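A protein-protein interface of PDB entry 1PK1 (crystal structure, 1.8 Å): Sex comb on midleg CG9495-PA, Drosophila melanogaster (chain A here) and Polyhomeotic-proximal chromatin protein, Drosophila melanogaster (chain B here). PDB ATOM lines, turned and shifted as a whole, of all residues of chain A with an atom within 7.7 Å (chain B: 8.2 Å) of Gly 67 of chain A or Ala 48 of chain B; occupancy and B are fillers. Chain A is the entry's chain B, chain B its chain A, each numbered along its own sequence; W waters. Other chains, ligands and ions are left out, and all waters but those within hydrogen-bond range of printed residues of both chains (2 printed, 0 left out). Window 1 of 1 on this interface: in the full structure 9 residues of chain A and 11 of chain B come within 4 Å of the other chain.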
ATOM      1  N   ASP A  30      12.251 -19.893 -33.559  1.00  0.00           N
ATOM      2  CA  ASP A  30      13.037 -19.215 -32.536  1.00  0.00           C
ATOM      3  C   ASP A  30      14.421 -18.924 -33.104  1.00  0.00           C
ATOM      4  O   ASP A  30      15.327 -19.751 -33.021  1.00  0.00           O
ATOM      5  CB  ASP A  30      13.164 -20.098 -31.291  1.00  0.00           C
ATOM      6  CG  ASP A  30      13.681 -19.339 -30.087  1.00  0.00           C
ATOM      7  OD1 ASP A  30      14.364 -18.310 -30.272  1.00  0.00           O
ATOM      8  OD2 ASP A  30      13.413 -19.783 -28.950  1.00  0.00           O
ATOM      9  N   LEU A  33      17.981 -19.660 -31.502  1.00  0.00           N
ATOM     10  CA  LEU A  33      18.510 -21.021 -31.434  1.00  0.00           C
ATOM     11  C   LEU A  33      19.300 -21.423 -32.680  1.00  0.00           C
ATOM     12  O   LEU A  33      19.889 -22.505 -32.724  1.00  0.00           O
ATOM     13  CB  LEU A  33      17.356 -22.008 -31.228  1.00  0.00           C
ATOM     14  CG  LEU A  33      16.663 -21.937 -29.865  1.00  0.00           C
ATOM     15  CD1 LEU A  33      15.390 -22.785 -29.898  1.00  0.00           C
ATOM     16  CD2 LEU A  33      17.620 -22.436 -28.781  1.00  0.00           C
ATOM     17  N   HIS A  36      22.781 -22.981 -32.768  1.00  0.00           N
ATOM     18  CA  HIS A  36      22.923 -24.398 -32.443  1.00  0.00           C
ATOM     19  C   HIS A  36      22.595 -25.316 -33.608  1.00  0.00           C
ATOM     20  O   HIS A  36      22.594 -26.537 -33.461  1.00  0.00           O
ATOM     21  CB  HIS A  36      22.031 -24.747 -31.246  1.00  0.00           C
ATOM     22  CG  HIS A  36      22.305 -23.914 -30.036  1.00  0.00           C
ATOM     23  ND1 HIS A  36      23.560 -23.806 -29.478  1.00  0.00           N
ATOM     24  CD2 HIS A  36      21.491 -23.131 -29.287  1.00  0.00           C
ATOM     25  CE1 HIS A  36      23.509 -22.992 -28.439  1.00  0.00           C
ATOM     26  NE2 HIS A  36      22.264 -22.569 -28.303  1.00  0.00           N
ATOM     27  N   MET A  59      21.634 -31.604 -22.525  1.00  0.00           N
ATOM     28  CA  MET A  59      22.705 -31.051 -21.713  1.00  0.00           C
ATOM     29  C   MET A  59      23.878 -32.008 -21.595  1.00  0.00           C
ATOM     30  O   MET A  59      25.028 -31.619 -21.762  1.00  0.00           O
ATOM     31  CB  MET A  59      22.186 -30.697 -20.319  1.00  0.00           C
ATOM     32  CG  MET A  59      21.157 -29.578 -20.316  1.00  0.00           C
ATOM     33  SD  MET A  59      20.754 -29.035 -18.646  1.00  0.00           S
ATOM     34  CE  MET A  59      19.786 -30.441 -18.064  1.00  0.00           C
ATOM     35  N   LEU A  64      24.397 -28.684 -24.678  1.00  0.00           N
ATOM     36  CA  LEU A  64      23.575 -27.478 -24.655  1.00  0.00           C
ATOM     37  C   LEU A  64      23.376 -27.029 -23.211  1.00  0.00           C
ATOM     38  O   LEU A  64      23.295 -27.858 -22.307  1.00  0.00           O
ATOM     39  CB  LEU A  64      22.211 -27.763 -25.290  1.00  0.00           C
ATOM     40  CG  LEU A  64      22.199 -27.927 -26.812  1.00  0.00           C
ATOM     41  CD1 LEU A  64      20.926 -28.612 -27.262  1.00  0.00           C
ATOM     42  CD2 LEU A  64      22.338 -26.550 -27.452  1.00  0.00           C
ATOM     43  N   LYS A  65      23.314 -25.719 -22.998  1.00  0.00           N
ATOM     44  CA  LYS A  65      23.074 -25.181 -21.663  1.00  0.00           C
ATOM     45  C   LYS A  65      21.567 -25.263 -21.402  1.00  0.00           C
ATOM     46  O   LYS A  65      20.783 -25.477 -22.333  1.00  0.00           O
ATOM     47  CB  LYS A  65      23.561 -23.731 -21.571  1.00  0.00           C
ATOM     48  CG  LYS A  65      25.061 -23.582 -21.801  1.00  0.00           C
ATOM     49  CD  LYS A  65      25.850 -24.509 -20.895  1.00  0.00           C
ATOM     50  CE  LYS A  65      27.352 -24.330 -21.093  1.00  0.00           C
ATOM     51  NZ  LYS A  65      28.128 -25.286 -20.273  1.00  0.00           N
ATOM     52  N   LEU A  66      21.162 -25.091 -20.146  1.00  0.00           N
ATOM     53  CA  LEU A  66      19.751 -25.204 -19.785  1.00  0.00           C
ATOM     54  C   LEU A  66      18.807 -24.268 -20.541  1.00  0.00           C
ATOM     55  O   LEU A  66      17.728 -24.688 -20.959  1.00  0.00           O
ATOM     56  CB  LEU A  66      19.579 -25.001 -18.275  1.00  0.00           C
ATOM     57  CG  LEU A  66      18.188 -25.243 -17.669  1.00  0.00           C
ATOM     58  CD1 LEU A  66      17.694 -26.633 -17.997  1.00  0.00           C
ATOM     59  CD2 LEU A  66      18.266 -25.050 -16.154  1.00  0.00           C
ATOM     60  N   GLY A  67      19.209 -23.008 -20.701  1.00  0.00           N
ATOM     61  CA  GLY A  67      18.371 -22.042 -21.400  1.00  0.00           C
ATOM     62  C   GLY A  67      17.950 -22.564 -22.757  1.00  0.00           C
ATOM     63  O   GLY A  67      16.757 -22.719 -23.046  1.00  0.00           O
ATOM     64  N   PRO A  68      18.926 -22.832 -23.628  1.00  0.00           N
ATOM     65  CA  PRO A  68      18.659 -23.351 -24.967  1.00  0.00           C
ATOM     66  C   PRO A  68      17.884 -24.671 -24.918  1.00  0.00           C
ATOM     67  O   PRO A  68      16.971 -24.891 -25.705  1.00  0.00           O
ATOM     68  CB  PRO A  68      20.060 -23.521 -25.546  1.00  0.00           C
ATOM     69  CG  PRO A  68      20.807 -22.391 -24.932  1.00  0.00           C
ATOM     70  CD  PRO A  68      20.334 -22.413 -23.496  1.00  0.00           C
ATOM     71  N   ALA A  69      18.240 -25.556 -23.987  1.00  0.00           N
ATOM     72  CA  ALA A  69      17.541 -26.837 -23.894  1.00  0.00           C
ATOM     73  C   ALA A  69      16.054 -26.644 -23.589  1.00  0.00           C
ATOM     74  O   ALA A  69      15.194 -27.300 -24.192  1.00  0.00           O
ATOM     75  CB  ALA A  69      18.189 -27.711 -22.823  1.00  0.00           C
ATOM     76  N   LEU A  70      15.748 -25.760 -22.646  1.00  0.00           N
ATOM     77  CA  LEU A  70      14.356 -25.511 -22.293  1.00  0.00           C
ATOM     78  C   LEU A  70      13.575 -24.908 -23.466  1.00  0.00           C
ATOM     79  O   LEU A  70      12.419 -25.262 -23.682  1.00  0.00           O
ATOM     80  CB  LEU A  70      14.262 -24.599 -21.069  1.00  0.00           C
ATOM     81  CG  LEU A  70      14.666 -25.249 -19.737  1.00  0.00           C
ATOM     82  CD1 LEU A  70      14.319 -24.310 -18.595  1.00  0.00           C
ATOM     83  CD2 LEU A  70      13.942 -26.575 -19.562  1.00  0.00           C
ATOM     84  N   LYS A  71      14.210 -24.016 -24.226  1.00  0.00           N
ATOM     85  CA  LYS A  71      13.542 -23.412 -25.377  1.00  0.00           C
ATOM     86  C   LYS A  71      13.274 -24.462 -26.451  1.00  0.00           C
ATOM     87  O   LYS A  71      12.226 -24.457 -27.097  1.00  0.00           O
ATOM     88  CB  LYS A  71      14.391 -22.290 -25.983  1.00  0.00           C
ATOM     89  CG  LYS A  71      14.606 -21.085 -25.094  1.00  0.00           C
ATOM     90  CD  LYS A  71      15.222 -19.970 -25.932  1.00  0.00           C
ATOM     91  CE  LYS A  71      16.334 -19.252 -25.221  1.00  0.00           C
ATOM     92  NZ  LYS A  71      17.047 -18.386 -26.205  1.00  0.00           N
ATOM     93  N   ILE A  72      14.231 -25.363 -26.650  1.00  0.00           N
ATOM     94  CA  ILE A  72      14.072 -26.406 -27.644  1.00  0.00           C
ATOM     95  C   ILE A  72      12.971 -27.366 -27.202  1.00  0.00           C
ATOM     96  O   ILE A  72      12.130 -27.762 -28.009  1.00  0.00           O
ATOM     97  CB  ILE A  72      15.402 -27.162 -27.865  1.00  0.00           C
ATOM     98  CG1 ILE A  72      16.408 -26.216 -28.543  1.00  0.00           C
ATOM     99  CG2 ILE A  72      15.162 -28.405 -28.707  1.00  0.00           C
ATOM    100  CD1 ILE A  72      17.847 -26.698 -28.520  1.00  0.00           C
ATOM    101  N   CYS A  73      12.959 -27.721 -25.920  1.00  0.00           N
ATOM    102  CA  CYS A  73      11.923 -28.625 -25.410  1.00  0.00           C
ATOM    103  C   CYS A  73      10.553 -27.999 -25.621  1.00  0.00           C
ATOM    104  O   CYS A  73       9.593 -28.695 -25.940  1.00  0.00           O
ATOM    105  CB  CYS A  73      12.114 -28.903 -23.917  1.00  0.00           C
ATOM    106  SG  CYS A  73      13.341 -30.149 -23.537  1.00  0.00           S
ATOM    107  N   ILE B  14       9.076  -9.733 -20.481  1.00  0.00           N
ATOM    108  CA  ILE B  14      10.199 -10.596 -20.142  1.00  0.00           C
ATOM    109  C   ILE B  14      10.624 -11.377 -21.383  1.00  0.00           C
ATOM    110  O   ILE B  14      11.806 -11.658 -21.580  1.00  0.00           O
ATOM    111  CB  ILE B  14       9.835 -11.574 -18.997  1.00  0.00           C
ATOM    112  CG1 ILE B  14       9.541 -10.774 -17.720  1.00  0.00           C
ATOM    113  CG2 ILE B  14      10.984 -12.563 -18.759  1.00  0.00           C
ATOM    114  CD1 ILE B  14       9.285 -11.620 -16.494  1.00  0.00           C
ATOM    115  N   SER B  15       9.655 -11.702 -22.234  1.00  0.00           N
ATOM    116  CA  SER B  15       9.942 -12.450 -23.451  1.00  0.00           C
ATOM    117  C   SER B  15      10.959 -11.735 -24.341  1.00  0.00           C
ATOM    118  O   SER B  15      11.563 -12.352 -25.210  1.00  0.00           O
ATOM    119  CB  SER B  15       8.648 -12.705 -24.232  1.00  0.00           C
ATOM    120  OG  SER B  15       7.992 -11.490 -24.545  1.00  0.00           O
ATOM    121  N   TRP B  17      13.529  -9.952 -22.952  1.00  0.00           N
ATOM    122  CA  TRP B  17      14.764  -9.832 -22.174  1.00  0.00           C
ATOM    123  C   TRP B  17      15.922 -10.654 -22.731  1.00  0.00           C
ATOM    124  O   TRP B  17      15.749 -11.802 -23.137  1.00  0.00           O
ATOM    125  CB  TRP B  17      14.527 -10.268 -20.725  1.00  0.00           C
ATOM    126  CG  TRP B  17      13.720  -9.324 -19.894  1.00  0.00           C
ATOM    127  CD1 TRP B  17      12.947  -8.288 -20.336  1.00  0.00           C
ATOM    128  CD2 TRP B  17      13.547  -9.378 -18.473  1.00  0.00           C
ATOM    129  NE1 TRP B  17      12.300  -7.696 -19.277  1.00  0.00           N
ATOM    130  CE2 TRP B  17      12.650  -8.347 -18.121  1.00  0.00           C
ATOM    131  CE3 TRP B  17      14.063 -10.200 -17.464  1.00  0.00           C
ATOM    132  CZ2 TRP B  17      12.253  -8.116 -16.797  1.00  0.00           C
ATOM    133  CZ3 TRP B  17      13.668  -9.971 -16.144  1.00  0.00           C
ATOM    134  CH2 TRP B  17      12.772  -8.937 -15.827  1.00  0.00           C
ATOM    135  N   VAL B  19      19.974 -12.214 -22.212  1.00  0.00           N
ATOM    136  CA  VAL B  19      20.625 -12.930 -21.122  1.00  0.00           C
ATOM    137  C   VAL B  19      21.138 -11.883 -20.124  1.00  0.00           C
ATOM    138  O   VAL B  19      21.111 -12.089 -18.913  1.00  0.00           O
ATOM    139  CB  VAL B  19      21.808 -13.780 -21.649  1.00  0.00           C
ATOM    140  CG1 VAL B  19      22.676 -14.265 -20.495  1.00  0.00           C
ATOM    141  CG2 VAL B  19      21.270 -14.981 -22.425  1.00  0.00           C
ATOM    142  N   VAL B  22      18.376 -10.601 -17.904  1.00  0.00           N
ATOM    143  CA  VAL B  22      18.087 -11.606 -16.883  1.00  0.00           C
ATOM    144  C   VAL B  22      19.160 -11.565 -15.801  1.00  0.00           C
ATOM    145  O   VAL B  22      18.855 -11.619 -14.607  1.00  0.00           O
ATOM    146  CB  VAL B  22      18.025 -13.027 -17.496  1.00  0.00           C
ATOM    147  CG1 VAL B  22      17.924 -14.081 -16.382  1.00  0.00           C
ATOM    148  CG2 VAL B  22      16.827 -13.128 -18.432  1.00  0.00           C
ATOM    149  N   PHE B  39      22.976 -18.344 -13.436  1.00  0.00           N
ATOM    150  CA  PHE B  39      22.180 -18.027 -14.609  1.00  0.00           C
ATOM    151  C   PHE B  39      23.019 -17.764 -15.851  1.00  0.00           C
ATOM    152  O   PHE B  39      22.676 -18.228 -16.932  1.00  0.00           O
ATOM    153  CB  PHE B  39      21.262 -16.836 -14.327  1.00  0.00           C
ATOM    154  CG  PHE B  39      20.040 -17.202 -13.535  1.00  0.00           C
ATOM    155  CD1 PHE B  39      20.148 -17.592 -12.202  1.00  0.00           C
ATOM    156  CD2 PHE B  39      18.786 -17.211 -14.141  1.00  0.00           C
ATOM    157  CE1 PHE B  39      19.018 -17.992 -11.480  1.00  0.00           C
ATOM    158  CE2 PHE B  39      17.651 -17.606 -13.434  1.00  0.00           C
ATOM    159  CZ  PHE B  39      17.770 -17.999 -12.096  1.00  0.00           C
ATOM    160  N   GLN B  41      25.884 -18.990 -16.606  1.00  0.00           N
ATOM    161  CA  GLN B  41      26.419 -20.274 -17.042  1.00  0.00           C
ATOM    162  C   GLN B  41      25.411 -21.046 -17.896  1.00  0.00           C
ATOM    163  O   GLN B  41      25.790 -21.783 -18.809  1.00  0.00           O
ATOM    164  CB  GLN B  41      26.799 -21.115 -15.815  1.00  0.00           C
ATOM    165  CG  GLN B  41      27.153 -22.563 -16.113  1.00  0.00           C
ATOM    166  CD  GLN B  41      27.372 -23.380 -14.851  1.00  0.00           C
ATOM    167  OE1 GLN B  41      26.459 -23.551 -14.044  1.00  0.00           O
ATOM    168  NE2 GLN B  41      28.589 -23.886 -14.674  1.00  0.00           N
ATOM    169  N   GLN B  42      24.127 -20.859 -17.612  1.00  0.00           N
ATOM    170  CA  GLN B  42      23.091 -21.579 -18.346  1.00  0.00           C
ATOM    171  C   GLN B  42      22.444 -20.829 -19.510  1.00  0.00           C
ATOM    172  O   GLN B  42      21.472 -21.307 -20.087  1.00  0.00           O
ATOM    173  CB  GLN B  42      22.012 -22.065 -17.375  1.00  0.00           C
ATOM    174  CG  GLN B  42      22.525 -23.037 -16.311  1.00  0.00           C
ATOM    175  CD  GLN B  42      23.363 -24.162 -16.898  1.00  0.00           C
ATOM    176  OE1 GLN B  42      22.995 -24.773 -17.903  1.00  0.00           O
ATOM    177  NE2 GLN B  42      24.500 -24.441 -16.268  1.00  0.00           N
ATOM    178  N   GLU B  43      22.987 -19.663 -19.853  1.00  0.00           N
ATOM    179  CA  GLU B  43      22.480 -18.863 -20.964  1.00  0.00           C
ATOM    180  C   GLU B  43      20.968 -18.655 -20.867  1.00  0.00           C
ATOM    181  O   GLU B  43      20.223 -18.926 -21.810  1.00  0.00           O
ATOM    182  CB  GLU B  43      22.851 -19.542 -22.290  1.00  0.00           C
ATOM    183  CG  GLU B  43      24.284 -20.101 -22.285  1.00  0.00           C
ATOM    184  CD  GLU B  43      24.725 -20.677 -23.626  1.00  0.00           C
ATOM    185  OE1 GLU B  43      23.902 -21.322 -24.308  1.00  0.00           O
ATOM    186  OE2 GLU B  43      25.907 -20.495 -23.990  1.00  0.00           O
ATOM    187  N   ILE B  44      20.524 -18.177 -19.710  1.00  0.00           N
ATOM    188  CA  ILE B  44      19.106 -17.929 -19.474  1.00  0.00           C
ATOM    189  C   ILE B  44      18.693 -16.538 -19.962  1.00  0.00           C
ATOM    190  O   ILE B  44      19.057 -15.529 -19.346  1.00  0.00           O
ATOM    191  CB  ILE B  44      18.760 -18.019 -17.964  1.00  0.00           C
ATOM    192  CG1 ILE B  44      19.195 -19.375 -17.387  1.00  0.00           C
ATOM    193  CG2 ILE B  44      17.250 -17.830 -17.762  1.00  0.00           C
ATOM    194  CD1 ILE B  44      18.506 -20.575 -18.018  1.00  0.00           C
ATOM    195  N   ASP B  45      17.972 -16.483 -21.080  1.00  0.00           N
ATOM    196  CA  ASP B  45      17.467 -15.211 -21.590  1.00  0.00           C
ATOM    197  C   ASP B  45      16.008 -15.109 -21.146  1.00  0.00           C
ATOM    198  O   ASP B  45      15.533 -15.950 -20.387  1.00  0.00           O
ATOM    199  CB  ASP B  45      17.581 -15.117 -23.120  1.00  0.00           C
ATOM    200  CG  ASP B  45      16.785 -16.190 -23.856  1.00  0.00           C
ATOM    201  OD1 ASP B  45      16.115 -17.033 -23.217  1.00  0.00           O
ATOM    202  OD2 ASP B  45      16.839 -16.184 -25.107  1.00  0.00           O
ATOM    203  N   GLY B  46      15.306 -14.078 -21.605  1.00  0.00           N
ATOM    204  CA  GLY B  46      13.920 -13.888 -21.205  1.00  0.00           C
ATOM    205  C   GLY B  46      12.999 -15.051 -21.511  1.00  0.00           C
ATOM    206  O   GLY B  46      12.182 -15.444 -20.672  1.00  0.00           O
ATOM    207  N   GLN B  47      13.116 -15.588 -22.720  1.00  0.00           N
ATOM    208  CA  GLN B  47      12.296 -16.716 -23.138  1.00  0.00           C
ATOM    209  C   GLN B  47      12.524 -17.893 -22.208  1.00  0.00           C
ATOM    210  O   GLN B  47      11.577 -18.534 -21.759  1.00  0.00           O
ATOM    211  CB  GLN B  47      12.651 -17.136 -24.564  1.00  0.00           C
ATOM    212  CG  GLN B  47      12.270 -16.145 -25.637  1.00  0.00           C
ATOM    213  CD  GLN B  47      12.477 -16.717 -27.024  1.00  0.00           C
ATOM    214  OE1 GLN B  47      11.870 -17.728 -27.386  1.00  0.00           O
ATOM    215  NE2 GLN B  47      13.340 -16.082 -27.806  1.00  0.00           N
ATOM    216  N   ALA B  48      13.792 -18.180 -21.931  1.00  0.00           N
ATOM    217  CA  ALA B  48      14.141 -19.288 -21.046  1.00  0.00           C
ATOM    218  C   ALA B  48      13.674 -19.027 -19.617  1.00  0.00           C
ATOM    219  O   ALA B  48      13.217 -19.944 -18.934  1.00  0.00           O
ATOM    220  CB  ALA B  48      15.646 -19.518 -21.066  1.00  0.00           C
ATOM    221  N   LEU B  49      13.789 -17.781 -19.165  1.00  0.00           N
ATOM    222  CA  LEU B  49      13.380 -17.440 -17.809  1.00  0.00           C
ATOM    223  C   LEU B  49      11.895 -17.749 -17.611  1.00  0.00           C
ATOM    224  O   LEU B  49      11.480 -18.219 -16.546  1.00  0.00           O
ATOM    225  CB  LEU B  49      13.665 -15.961 -17.522  1.00  0.00           C
ATOM    226  CG  LEU B  49      13.364 -15.493 -16.092  1.00  0.00           C
ATOM    227  CD1 LEU B  49      14.272 -16.232 -15.114  1.00  0.00           C
ATOM    228  CD2 LEU B  49      13.582 -13.990 -15.978  1.00  0.00           C
ATOM    229  N   LEU B  50      11.093 -17.486 -18.637  1.00  0.00           N
ATOM    230  CA  LEU B  50       9.659 -17.765 -18.568  1.00  0.00           C
ATOM    231  C   LEU B  50       9.375 -19.264 -18.468  1.00  0.00           C
ATOM    232  O   LEU B  50       8.353 -19.676 -17.909  1.00  0.00           O
ATOM    233  CB  LEU B  50       8.952 -17.198 -19.802  1.00  0.00           C
ATOM    234  CG  LEU B  50       8.897 -15.672 -19.881  1.00  0.00           C
ATOM    235  CD1 LEU B  50       8.474 -15.249 -21.277  1.00  0.00           C
ATOM    236  CD2 LEU B  50       7.929 -15.143 -18.824  1.00  0.00           C
ATOM    237  N   LEU B  51      10.284 -20.078 -19.007  1.00  0.00           N
ATOM    238  CA  LEU B  51      10.131 -21.532 -18.996  1.00  0.00           C
ATOM    239  C   LEU B  51      10.788 -22.189 -17.788  1.00  0.00           C
ATOM    240  O   LEU B  51      10.554 -23.363 -17.509  1.00  0.00           O
ATOM    241  CB  LEU B  51      10.748 -22.134 -20.264  1.00  0.00           C
ATOM    242  CG  LEU B  51      10.194 -21.625 -21.598  1.00  0.00           C
ATOM    243  CD1 LEU B  51      11.081 -22.111 -22.743  1.00  0.00           C
ATOM    244  CD2 LEU B  51       8.766 -22.117 -21.775  1.00  0.00           C
ATOM    245  N   LEU B  52      11.609 -21.428 -17.075  1.00  0.00           N
ATOM    246  CA  LEU B  52      12.335 -21.941 -15.920  1.00  0.00           C
ATOM    247  C   LEU B  52      11.426 -22.128 -14.705  1.00  0.00           C
ATOM    248  O   LEU B  52      10.845 -21.172 -14.204  1.00  0.00           O
ATOM    249  CB  LEU B  52      13.481 -20.977 -15.588  1.00  0.00           C
ATOM    250  CG  LEU B  52      14.646 -21.410 -14.699  1.00  0.00           C
ATOM    251  CD1 LEU B  52      15.344 -22.638 -15.281  1.00  0.00           C
ATOM    252  CD2 LEU B  52      15.625 -20.246 -14.598  1.00  0.00           C
ATOM    253  N   LYS B  53      11.304 -23.365 -14.238  1.00  0.00           N
ATOM    254  CA  LYS B  53      10.469 -23.652 -13.079  1.00  0.00           C
ATOM    255  C   LYS B  53      11.284 -24.277 -11.950  1.00  0.00           C
ATOM    256  O   LYS B  53      12.443 -24.641 -12.133  1.00  0.00           O
ATOM    257  CB  LYS B  53       9.314 -24.573 -13.484  1.00  0.00           C
ATOM    258  CG  LYS B  53       8.443 -23.999 -14.593  1.00  0.00           C
ATOM    259  CD  LYS B  53       7.884 -22.628 -14.221  1.00  0.00           C
ATOM    260  CE  LYS B  53       7.150 -21.988 -15.397  1.00  0.00           C
ATOM    261  NZ  LYS B  53       6.664 -20.619 -15.063  1.00  0.00           N
ATOM    262  N   HIS B  56      13.547 -27.252 -12.529  1.00  0.00           N
ATOM    263  CA  HIS B  56      14.780 -26.980 -13.264  1.00  0.00           C
ATOM    264  C   HIS B  56      15.834 -26.325 -12.381  1.00  0.00           C
ATOM    265  O   HIS B  56      16.990 -26.730 -12.382  1.00  0.00           O
ATOM    266  CB  HIS B  56      14.496 -26.069 -14.465  1.00  0.00           C
ATOM    267  CG  HIS B  56      13.442 -26.594 -15.387  1.00  0.00           C
ATOM    268  ND1 HIS B  56      12.239 -25.950 -15.583  1.00  0.00           N
ATOM    269  CD2 HIS B  56      13.403 -27.707 -16.155  1.00  0.00           C
ATOM    270  CE1 HIS B  56      11.503 -26.646 -16.431  1.00  0.00           C
ATOM    271  NE2 HIS B  56      12.187 -27.717 -16.792  1.00  0.00           N
ATOM    272  N   MET B  61      19.957 -27.030 -11.769  1.00  0.00           N
ATOM    273  CA  MET B  61      20.910 -26.008 -11.360  1.00  0.00           C
ATOM    274  C   MET B  61      21.341 -26.138  -9.898  1.00  0.00           C
ATOM    275  O   MET B  61      22.162 -25.366  -9.415  1.00  0.00           O
ATOM    276  CB  MET B  61      20.315 -24.623 -11.645  1.00  0.00           C
ATOM    277  CG  MET B  61      20.102 -24.381 -13.135  1.00  0.00           C
ATOM    278  SD  MET B  61      19.230 -22.720 -13.579  1.00  0.00           S
ATOM    279  CE  MET B  61      20.136 -21.595 -12.266  1.00  0.00           C
ATOM    280  N   VAL B  75       9.172 -13.850 -11.154  1.00  0.00           N
ATOM    281  CA  VAL B  75       8.991 -13.810 -12.596  1.00  0.00           C
ATOM    282  C   VAL B  75       7.507 -13.735 -12.951  1.00  0.00           C
ATOM    283  O   VAL B  75       7.097 -12.866 -13.719  1.00  0.00           O
ATOM    284  CB  VAL B  75       9.629 -15.046 -13.268  1.00  0.00           C
ATOM    285  CG1 VAL B  75       9.233 -15.112 -14.728  1.00  0.00           C
ATOM    286  CG2 VAL B  75      11.146 -14.969 -13.137  1.00  0.00           C
HETATM  287  O   HOH W   1      24.137 -24.045 -25.163  1.00  0.00           O
HETATM  288  O   HOH W   2      19.664 -18.332 -24.302  1.00  0.00           O
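The backbone NH of Leu 66 of chain A is in hydrogen-bond range of the side-chain amide oxygen of Gln 42 of chain B, at 2.9 Å.
The backbone carbonyl oxygen (O) of Gln 42 of chain B sits at hydrogen-bond distance from the backbone NH (N) of Gly 67 of chain A (2.9 Å).
NZ of Lys 71 of chain A is in salt-bridge range of OD2 of Asp 45 of chain B (2.5 Å).
The side-chain carboxylate of Asp 30 of chain A lies close to the side-chain amide oxygen of Gln 47 of chain B (3.0 Å).
The side-chain amide oxygen (OE1) of Gln 41 of chain B lies within hydrogen-bond range of the side-chain amide nitrogen (NE2) of Gln 42 of chain B, at 3.1 Å.
The side-chain carboxylate of Asp 45 of chain B lies close to the backbone NH of Gln 47 of chain B (3.4 Å).
The side-chain carboxylate (OD1) of Asp 45 of chain B lies within hydrogen-bond range of the backbone NH (N) of Ala 48 of chain B (2.9 Å).
ND1 of His 56 of chain B is in hydrogen-bond range of N of Lys 53 of chain B.
The backbone carbonyl oxygen (O) of His 56 of chain B sits at hydrogen-bond distance from the backbone NH (N) of Met 61 of chain B, at 3.0 Å.
Lys 65 of chain A touches Gln 41 of chain B.
Gln 42 of chain B touches Lys 65 of chain A (O to CB, 3.5 Å).
Leu 52 of chain B touches Leu 66 of chain A (CD1 to CD2, 3.9 Å).
Leu 66 of chain A touches Met 61 of chain B (CD2 to CG, 3.6 Å).
Glu 43 of chain B touches Gly 67 of chain A (O to CA, 3.6 Å).
CA of Gly 67 of chain A touches CD1 of Ile 44 of chain B (3.7 Å).
Pro 68 of chain A touches Gln 42 of chain B (CD to O, 3.8 Å).
Glu 43 of chain B touches Pro 68 of chain A (OE1 to CG, 3.3 Å).
Leu 70 of chain A touches Leu 51 of chain B.
Leu 70 of chain A touches His 56 of chain B.
Pro 68 of chain A touches two residues of chain B.
Printed residues of chain B within 4 Å of Lys 65 of chain A: Gln 41 (3.4 Å), Gln 42 (3.5 Å) and Glu 43 (3.4 Å).
Of the printed residues of chain A, Gln 41 of chain B touches Lys 65 (3.4 Å).
Printed residues of chain A within 4 Å of Met 61 of chain B: Leu 66.
Printed residues of chain B within 4 Å of Lys 71 of chain A: Asp 45 (2.5 Å) and Leu 51 (3.8 Å).
Ser 15 of chain B touches none of the printed residues of chain A.
The nearest residue of chain B that does not touch Gly 67 of chain A is Asp 45 of chain B (5.6 Å).
The nearest residue of chain A that does not touch Ala 48 of chain B is Lys 71 of chain A (4.2 Å).
Printed residues of chain B that touch a printed residue of chain A: Gln 41, Gln 42, Glu 43, Ile 44, Asp 45, Gln 47, Ala 48, Leu 51, Leu 52, His 56 and Met 61.
Among the printed residues, Asp or Glu carboxylates within 4 Å of a Lys or Arg side-chain nitrogen of the other chain: Lys 71 of chain A with Asp 45 of chain B (2.5 Å).
Water W2 lies within hydrogen-bond range of the backbone carbonyl oxygen (O) of Glu 43 of chain B (2.6 Å) and the side-chain amino group (NZ) of Lys 71 of chain A (3.2 Å).
Water W1 bridges the backbone NH (N) of Lys 65 of chain A and the side-chain carboxylate (OE1) of Glu 43 of chain B.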
